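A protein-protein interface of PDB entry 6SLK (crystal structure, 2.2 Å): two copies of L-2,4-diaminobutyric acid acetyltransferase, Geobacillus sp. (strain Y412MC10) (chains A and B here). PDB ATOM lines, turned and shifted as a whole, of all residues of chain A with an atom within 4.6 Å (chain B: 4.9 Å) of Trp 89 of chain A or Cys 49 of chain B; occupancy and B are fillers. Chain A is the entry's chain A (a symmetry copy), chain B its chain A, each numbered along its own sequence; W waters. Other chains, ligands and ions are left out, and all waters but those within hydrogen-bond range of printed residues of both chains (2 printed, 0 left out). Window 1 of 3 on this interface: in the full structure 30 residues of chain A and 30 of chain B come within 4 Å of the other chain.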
ATOM      1  N   ASN A  45     -24.273 -22.775  -5.024  1.00  0.00           N
ATOM      2  CA  ASN A  45     -25.441 -23.330  -4.334  1.00  0.00           C
ATOM      3  C   ASN A  45     -25.592 -22.724  -2.911  1.00  0.00           C
ATOM      4  O   ASN A  45     -24.790 -21.897  -2.508  1.00  0.00           O
ATOM      5  CB  ASN A  45     -25.329 -24.836  -4.354  1.00  0.00           C
ATOM      6  CG  ASN A  45     -25.237 -25.374  -5.780  1.00  0.00           C
ATOM      7  OD1 ASN A  45     -24.212 -25.914  -6.237  1.00  0.00           O
ATOM      8  ND2 ASN A  45     -26.263 -25.182  -6.485  1.00  0.00           N
ATOM      9  N   CYS A  49     -26.754 -26.751   0.967  1.00  0.00           N
ATOM     10  CA  CYS A  49     -26.348 -27.753  -0.048  1.00  0.00           C
ATOM     11  C   CYS A  49     -24.963 -28.285   0.276  1.00  0.00           C
ATOM     12  O   CYS A  49     -24.707 -29.555   0.281  1.00  0.00           O
ATOM     13  CB  CYS A  49     -26.381 -27.128  -1.444  1.00  0.00           C
ATOM     14  SG  CYS A  49     -25.813 -28.240  -2.711  1.00  0.00           S
ATOM     15  N   LEU A  53     -23.719 -32.064   1.320  1.00  0.00           N
ATOM     16  CA  LEU A  53     -22.637 -32.764   0.659  1.00  0.00           C
ATOM     17  C   LEU A  53     -21.603 -33.253   1.676  1.00  0.00           C
ATOM     18  O   LEU A  53     -21.127 -34.448   1.627  1.00  0.00           O
ATOM     19  CB  LEU A  53     -21.958 -31.842  -0.375  1.00  0.00           C
ATOM     20  CG  LEU A  53     -22.799 -31.540  -1.614  1.00  0.00           C
ATOM     21  CD1 LEU A  53     -22.183 -30.427  -2.461  1.00  0.00           C
ATOM     22  CD2 LEU A  53     -22.920 -32.794  -2.451  1.00  0.00           C
ATOM     23  N   SER A  75     -16.867 -31.803  -5.397  1.00  0.00           N
ATOM     24  CA  SER A  75     -18.079 -32.531  -5.073  1.00  0.00           C
ATOM     25  C   SER A  75     -18.379 -33.598  -6.136  1.00  0.00           C
ATOM     26  O   SER A  75     -18.243 -33.320  -7.325  1.00  0.00           O
ATOM     27  CB  SER A  75     -19.248 -31.525  -4.939  1.00  0.00           C
ATOM     28  OG  SER A  75     -19.465 -30.721  -6.056  1.00  0.00           O
ATOM     29  N   ALA A  76     -18.764 -34.810  -5.718  1.00  0.00           N
ATOM     30  CA  ALA A  76     -19.158 -35.803  -6.658  1.00  0.00           C
ATOM     31  C   ALA A  76     -20.127 -36.746  -6.022  1.00  0.00           C
ATOM     32  O   ALA A  76     -20.221 -36.814  -4.808  1.00  0.00           O
ATOM     33  CB  ALA A  76     -17.949 -36.595  -7.187  1.00  0.00           C
ATOM     34  N   PHE A  77     -20.813 -37.494  -6.865  1.00  0.00           N
ATOM     35  CA  PHE A  77     -21.655 -38.587  -6.402  1.00  0.00           C
ATOM     36  C   PHE A  77     -21.705 -39.686  -7.406  1.00  0.00           C
ATOM     37  O   PHE A  77     -21.546 -39.438  -8.558  1.00  0.00           O
ATOM     38  CB  PHE A  77     -23.098 -38.096  -6.158  1.00  0.00           C
ATOM     39  CG  PHE A  77     -23.721 -37.367  -7.334  1.00  0.00           C
ATOM     40  CD1 PHE A  77     -24.413 -38.067  -8.323  1.00  0.00           C
ATOM     41  CD2 PHE A  77     -23.626 -36.016  -7.437  1.00  0.00           C
ATOM     42  CE1 PHE A  77     -24.976 -37.411  -9.412  1.00  0.00           C
ATOM     43  CE2 PHE A  77     -24.199 -35.363  -8.510  1.00  0.00           C
ATOM     44  CZ  PHE A  77     -24.878 -36.054  -9.493  1.00  0.00           C
ATOM     45  N   PHE A  87     -20.282 -39.073 -11.138  1.00  0.00           N
ATOM     46  CA  PHE A  87     -20.472 -37.763 -11.640  1.00  0.00           C
ATOM     47  C   PHE A  87     -19.754 -36.748 -10.781  1.00  0.00           C
ATOM     48  O   PHE A  87     -20.005 -36.669  -9.590  1.00  0.00           O
ATOM     49  CB  PHE A  87     -21.976 -37.415 -11.658  1.00  0.00           C
ATOM     50  CG  PHE A  87     -22.250 -36.114 -12.311  1.00  0.00           C
ATOM     51  CD1 PHE A  87     -22.435 -36.061 -13.689  1.00  0.00           C
ATOM     52  CD2 PHE A  87     -22.233 -34.967 -11.609  1.00  0.00           C
ATOM     53  CE1 PHE A  87     -22.643 -34.859 -14.342  1.00  0.00           C
ATOM     54  CE2 PHE A  87     -22.492 -33.731 -12.237  1.00  0.00           C
ATOM     55  CZ  PHE A  87     -22.674 -33.676 -13.609  1.00  0.00           C
ATOM     56  N   VAL A  88     -18.889 -35.926 -11.382  1.00  0.00           N
ATOM     57  CA  VAL A  88     -18.167 -34.879 -10.706  1.00  0.00           C
ATOM     58  C   VAL A  88     -18.924 -33.600 -10.995  1.00  0.00           C
ATOM     59  O   VAL A  88     -19.146 -33.196 -12.154  1.00  0.00           O
ATOM     60  CB  VAL A  88     -16.713 -34.790 -11.192  1.00  0.00           C
ATOM     61  CG1 VAL A  88     -15.986 -33.616 -10.543  1.00  0.00           C
ATOM     62  CG2 VAL A  88     -15.994 -36.097 -10.896  1.00  0.00           C
ATOM     63  N   TRP A  89     -19.407 -33.026  -9.907  1.00  0.00           N
ATOM     64  CA  TRP A  89     -20.222 -31.848  -9.909  1.00  0.00           C
ATOM     65  C   TRP A  89     -19.377 -30.544  -9.943  1.00  0.00           C
ATOM     66  O   TRP A  89     -19.337 -29.915 -10.965  1.00  0.00           O
ATOM     67  CB  TRP A  89     -21.244 -31.936  -8.759  1.00  0.00           C
ATOM     68  CG  TRP A  89     -22.236 -30.816  -8.632  1.00  0.00           C
ATOM     69  CD1 TRP A  89     -22.331 -29.654  -9.402  1.00  0.00           C
ATOM     70  CD2 TRP A  89     -23.297 -30.724  -7.662  1.00  0.00           C
ATOM     71  NE1 TRP A  89     -23.364 -28.878  -8.940  1.00  0.00           N
ATOM     72  CE2 TRP A  89     -23.971 -29.508  -7.883  1.00  0.00           C
ATOM     73  CE3 TRP A  89     -23.727 -31.545  -6.609  1.00  0.00           C
ATOM     74  CZ2 TRP A  89     -25.068 -29.115  -7.103  1.00  0.00           C
ATOM     75  CZ3 TRP A  89     -24.817 -31.140  -5.819  1.00  0.00           C
ATOM     76  CH2 TRP A  89     -25.474 -29.949  -6.090  1.00  0.00           C
ATOM     77  N   GLN A  90     -18.786 -30.109  -8.842  1.00  0.00           N
ATOM     78  CA  GLN A  90     -17.983 -28.875  -8.798  1.00  0.00           C
ATOM     79  C   GLN A  90     -16.525 -29.123  -8.482  1.00  0.00           C
ATOM     80  O   GLN A  90     -16.186 -30.019  -7.692  1.00  0.00           O
ATOM     81  CB  GLN A  90     -18.551 -27.871  -7.833  1.00  0.00           C
ATOM     82  CG  GLN A  90     -19.925 -27.391  -8.240  1.00  0.00           C
ATOM     83  CD  GLN A  90     -20.391 -26.198  -7.424  1.00  0.00           C
ATOM     84  OE1 GLN A  90     -20.878 -26.308  -6.264  1.00  0.00           O
ATOM     85  NE2 GLN A  90     -20.255 -25.034  -8.028  1.00  0.00           N
ATOM     86  N   VAL A  91     -15.663 -28.373  -9.149  1.00  0.00           N
ATOM     87  CA  VAL A  91     -14.230 -28.313  -8.812  1.00  0.00           C
ATOM     88  C   VAL A  91     -13.891 -26.850  -8.598  1.00  0.00           C
ATOM     89  O   VAL A  91     -14.242 -26.014  -9.423  1.00  0.00           O
ATOM     90  CB  VAL A  91     -13.358 -28.868  -9.952  1.00  0.00           C
ATOM     91  CG1 VAL A  91     -11.878 -28.854  -9.591  1.00  0.00           C
ATOM     92  CG2 VAL A  91     -13.790 -30.267 -10.290  1.00  0.00           C
ATOM     93  N   ASN B  45     -30.961 -23.068  -4.442  1.00  0.00           N
ATOM     94  CA  ASN B  45     -29.747 -23.536  -5.116  1.00  0.00           C
ATOM     95  C   ASN B  45     -29.649 -22.962  -6.557  1.00  0.00           C
ATOM     96  O   ASN B  45     -30.522 -22.223  -6.984  1.00  0.00           O
ATOM     97  CB  ASN B  45     -29.724 -25.044  -5.050  1.00  0.00           C
ATOM     98  CG  ASN B  45     -29.769 -25.545  -3.608  1.00  0.00           C
ATOM     99  OD1 ASN B  45     -30.742 -26.161  -3.134  1.00  0.00           O
ATOM    100  ND2 ASN B  45     -28.765 -25.240  -2.911  1.00  0.00           N
ATOM    101  N   SER B  46     -28.550 -23.275  -7.267  1.00  0.00           N
ATOM    102  CA  SER B  46     -28.274 -22.793  -8.605  1.00  0.00           C
ATOM    103  C   SER B  46     -29.191 -23.505  -9.576  1.00  0.00           C
ATOM    104  O   SER B  46     -29.656 -24.698  -9.351  1.00  0.00           O
ATOM    105  CB  SER B  46     -26.799 -23.059  -8.984  1.00  0.00           C
ATOM    106  OG  SER B  46     -26.594 -24.453  -9.282  1.00  0.00           O
ATOM    107  N   PRO B  47     -29.494 -22.819 -10.677  1.00  0.00           N
ATOM    108  CA  PRO B  47     -30.301 -23.524 -11.673  1.00  0.00           C
ATOM    109  C   PRO B  47     -29.722 -24.903 -12.116  1.00  0.00           C
ATOM    110  O   PRO B  47     -30.464 -25.873 -12.258  1.00  0.00           O
ATOM    111  CB  PRO B  47     -30.427 -22.492 -12.798  1.00  0.00           C
ATOM    112  CG  PRO B  47     -30.164 -21.133 -12.158  1.00  0.00           C
ATOM    113  CD  PRO B  47     -29.197 -21.420 -11.040  1.00  0.00           C
ATOM    114  N   TYR B  48     -28.409 -24.970 -12.267  1.00  0.00           N
ATOM    115  CA  TYR B  48     -27.728 -26.179 -12.588  1.00  0.00           C
ATOM    116  C   TYR B  48     -28.055 -27.317 -11.614  1.00  0.00           C
ATOM    117  O   TYR B  48     -28.231 -28.502 -12.020  1.00  0.00           O
ATOM    118  CB  TYR B  48     -26.202 -25.893 -12.568  1.00  0.00           C
ATOM    119  CG  TYR B  48     -25.346 -27.037 -13.093  1.00  0.00           C
ATOM    120  CD1 TYR B  48     -25.178 -27.273 -14.468  1.00  0.00           C
ATOM    121  CD2 TYR B  48     -24.707 -27.892 -12.212  1.00  0.00           C
ATOM    122  CE1 TYR B  48     -24.402 -28.347 -14.926  1.00  0.00           C
ATOM    123  CE2 TYR B  48     -23.897 -28.929 -12.643  1.00  0.00           C
ATOM    124  CZ  TYR B  48     -23.753 -29.181 -13.992  1.00  0.00           C
ATOM    125  OH  TYR B  48     -22.945 -30.264 -14.330  1.00  0.00           O
ATOM    126  N   CYS B  49     -28.125 -26.985 -10.312  1.00  0.00           N
ATOM    127  CA  CYS B  49     -28.441 -27.988  -9.267  1.00  0.00           C
ATOM    128  C   CYS B  49     -29.772 -28.651  -9.572  1.00  0.00           C
ATOM    129  O   CYS B  49     -29.913 -29.939  -9.539  1.00  0.00           O
ATOM    130  CB  CYS B  49     -28.466 -27.320  -7.890  1.00  0.00           C
ATOM    131  SG  CYS B  49     -28.933 -28.439  -6.590  1.00  0.00           S
ATOM    132  N   TYR B  50     -30.749 -27.809  -9.960  1.00  0.00           N
ATOM    133  CA  TYR B  50     -32.096 -28.334 -10.239  1.00  0.00           C
ATOM    134  C   TYR B  50     -32.132 -29.200 -11.506  1.00  0.00           C
ATOM    135  O   TYR B  50     -32.858 -30.257 -11.577  1.00  0.00           O
ATOM    136  CB  TYR B  50     -33.202 -27.237 -10.164  1.00  0.00           C
ATOM    137  CG  TYR B  50     -33.268 -26.640  -8.772  1.00  0.00           C
ATOM    138  CD1 TYR B  50     -33.766 -27.377  -7.697  1.00  0.00           C
ATOM    139  CD2 TYR B  50     -32.778 -25.373  -8.507  1.00  0.00           C
ATOM    140  CE1 TYR B  50     -33.751 -26.859  -6.397  1.00  0.00           C
ATOM    141  CE2 TYR B  50     -32.775 -24.838  -7.233  1.00  0.00           C
ATOM    142  CZ  TYR B  50     -33.276 -25.569  -6.162  1.00  0.00           C
ATOM    143  OH  TYR B  50     -33.253 -25.026  -4.875  1.00  0.00           O
ATOM    144  N   MET B  51     -31.261 -28.853 -12.439  1.00  0.00           N
ATOM    145  CA  MET B  51     -31.103 -29.687 -13.663  1.00  0.00           C
ATOM    146  C   MET B  51     -30.507 -31.053 -13.359  1.00  0.00           C
ATOM    147  O   MET B  51     -31.015 -32.060 -13.862  1.00  0.00           O
ATOM    148  CB  MET B  51     -30.225 -28.993 -14.688  1.00  0.00           C
ATOM    149  CG  MET B  51     -30.872 -27.819 -15.389  1.00  0.00           C
ATOM    150  SD  MET B  51     -29.609 -26.990 -16.435  1.00  0.00           S
ATOM    151  CE  MET B  51     -30.395 -25.377 -16.483  1.00  0.00           C
ATOM    152  N   LEU B  52     -29.474 -31.076 -12.506  1.00  0.00           N
ATOM    153  CA  LEU B  52     -28.880 -32.321 -12.072  1.00  0.00           C
ATOM    154  C   LEU B  52     -29.862 -33.176 -11.361  1.00  0.00           C
ATOM    155  O   LEU B  52     -29.875 -34.408 -11.562  1.00  0.00           O
ATOM    156  CB  LEU B  52     -27.764 -32.090 -11.049  1.00  0.00           C
ATOM    157  CG  LEU B  52     -26.423 -31.549 -11.545  1.00  0.00           C
ATOM    158  CD1 LEU B  52     -25.477 -31.628 -10.383  1.00  0.00           C
ATOM    159  CD2 LEU B  52     -25.866 -32.330 -12.752  1.00  0.00           C
ATOM    160  N   LEU B  53     -30.670 -32.557 -10.499  1.00  0.00           N
ATOM    161  CA  LEU B  53     -31.686 -33.331  -9.816  1.00  0.00           C
ATOM    162  C   LEU B  53     -32.670 -33.942 -10.816  1.00  0.00           C
ATOM    163  O   LEU B  53     -33.037 -35.173 -10.730  1.00  0.00           O
ATOM    164  CB  LEU B  53     -32.446 -32.443  -8.810  1.00  0.00           C
ATOM    165  CG  LEU B  53     -31.637 -32.029  -7.581  1.00  0.00           C
ATOM    166  CD1 LEU B  53     -32.352 -30.950  -6.768  1.00  0.00           C
ATOM    167  CD2 LEU B  53     -31.406 -33.241  -6.707  1.00  0.00           C
ATOM    168  N   TRP B  89     -34.894 -33.560   0.758  1.00  0.00           N
ATOM    169  CA  TRP B  89     -34.187 -32.314   0.723  1.00  0.00           C
ATOM    170  C   TRP B  89     -35.146 -31.091   0.718  1.00  0.00           C
ATOM    171  O   TRP B  89     -35.244 -30.438   1.721  1.00  0.00           O
ATOM    172  CB  TRP B  89     -33.160 -32.346  -0.426  1.00  0.00           C
ATOM    173  CG  TRP B  89     -32.273 -31.145  -0.588  1.00  0.00           C
ATOM    174  CD1 TRP B  89     -32.284 -29.956   0.146  1.00  0.00           C
ATOM    175  CD2 TRP B  89     -31.223 -30.988  -1.562  1.00  0.00           C
ATOM    176  NE1 TRP B  89     -31.324 -29.105  -0.340  1.00  0.00           N
ATOM    177  CE2 TRP B  89     -30.662 -29.711  -1.379  1.00  0.00           C
ATOM    178  CE3 TRP B  89     -30.720 -31.799  -2.590  1.00  0.00           C
ATOM    179  CZ2 TRP B  89     -29.603 -29.244  -2.172  1.00  0.00           C
ATOM    180  CZ3 TRP B  89     -29.669 -31.322  -3.394  1.00  0.00           C
ATOM    181  CH2 TRP B  89     -29.123 -30.068  -3.160  1.00  0.00           C
HETATM  182  O   HOH W   1     -24.037 -25.839  -9.276  1.00  0.00           O
HETATM  183  O   HOH W   2     -20.427 -31.124 -13.758  1.00  0.00           O
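ND2 of Asn 45 of chain A sits at hydrogen-bond distance from OG of Ser 46 of chain B, at 2.9 Å.
N of Asn 45 of chain B lies within hydrogen-bond range of OH of Tyr 50 of chain B (3.0 Å).
The side-chain hydroxyl of Ser 46 of chain B lies within hydrogen-bond range of the backbone NH of Cys 49 of chain B, 3.1 Å away.
OD1 of Asn 45 of chain A lies close to OE1 of Gln 90 of chain A (3.4 Å).
The backbone carbonyl oxygen of Ser 75 of chain A is in hydrogen-bond range of the backbone NH of Trp 89 of chain A (2.8 Å).
The backbone carbonyl oxygen (O) of Phe 77 of chain A sits at hydrogen-bond distance from the backbone NH (N) of Phe 87 of chain A (2.9 Å).
Among the printed residues, merely in contact across the chains: Asn 45 of chain A with Asn 45 of chain B (3.7 Å), Asn 45 of chain A with Cys 49 of chain B (3.4 Å), Cys 49 of chain A with Asn 45 of chain B (3.4 Å), Cys 49 of chain A with Trp 89 of chain B (3.8 Å), Phe 87 of chain A with Tyr 48 of chain B (3.5 Å), Phe 87 of chain A with Leu 52 of chain B (3.6 Å), Trp 89 of chain A with Tyr 48 of chain B (3.7 Å), Trp 89 of chain A with Cys 49 of chain B (3.8 Å) and Trp 89 of chain A with Leu 52 of chain B (3.6 Å).
Cys 49 of chain B touches just these residues of chain A: Asn 45 (3.4 Å) and Trp 89 (3.8 Å).
Printed residues of chain B within 4 Å of Phe 87 of chain A: Tyr 48 and Leu 52.
Of the printed residues of chain B, Cys 49 of chain A touches Asn 45 and Trp 89.
Of the printed residues of chain A, Asn 45 of chain B touches Asn 45 and Cys 49.
Of the printed residues of chain A, Trp 89 of chain B touches Cys 49.
Pro 47 of chain B touches none of the printed residues of chain A.
The nearest residue of chain B that does not touch Trp 89 of chain A is Trp 89 of chain B (4.7 Å).
Hydrophobic or aromatic side chains of chain B that line the printed part of chain A: Tyr 48, Leu 52 and Trp 89.
Hydrophobic or aromatic side chains of chain A within 4 Å of the printed part of chain B: Phe 87 and Trp 89.
Among the printed residues, 10 pairs touch across the chains.
Among the printed residues, no Asp or Glu carboxylate lies within 4 Å of a Lys or Arg side-chain nitrogen of the other chain.
Asn 45 of chain B touches its own counterpart, Asn 45 of chain A.
Asn 45 of chain A touches Cys 49 of chain B, and with the chains exchanged Cys 49 of chain A touches Asn 45 of chain B.
Cys 49 of chain A touches Trp 89 of chain B, and with the chains exchanged Trp 89 of chain A touches Cys 49 of chain B.
Water W2 lies within hydrogen-bond range of the side-chain hydroxyl (OH) of Tyr 48 of chain B (2.7 Å), the backbone carbonyl oxygen (O) of Val 88 of chain A (2.9 Å) and the backbone carbonyl oxygen (O) of Trp 89 of chain A (3.2 Å).
Water W1 lies within hydrogen-bond range of OG of Ser 46 of chain B (2.9 Å), OD1 of Asn 45 of chain A (3.0 Å) and NE1 of Trp 89 of chain A (3.1 Å).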
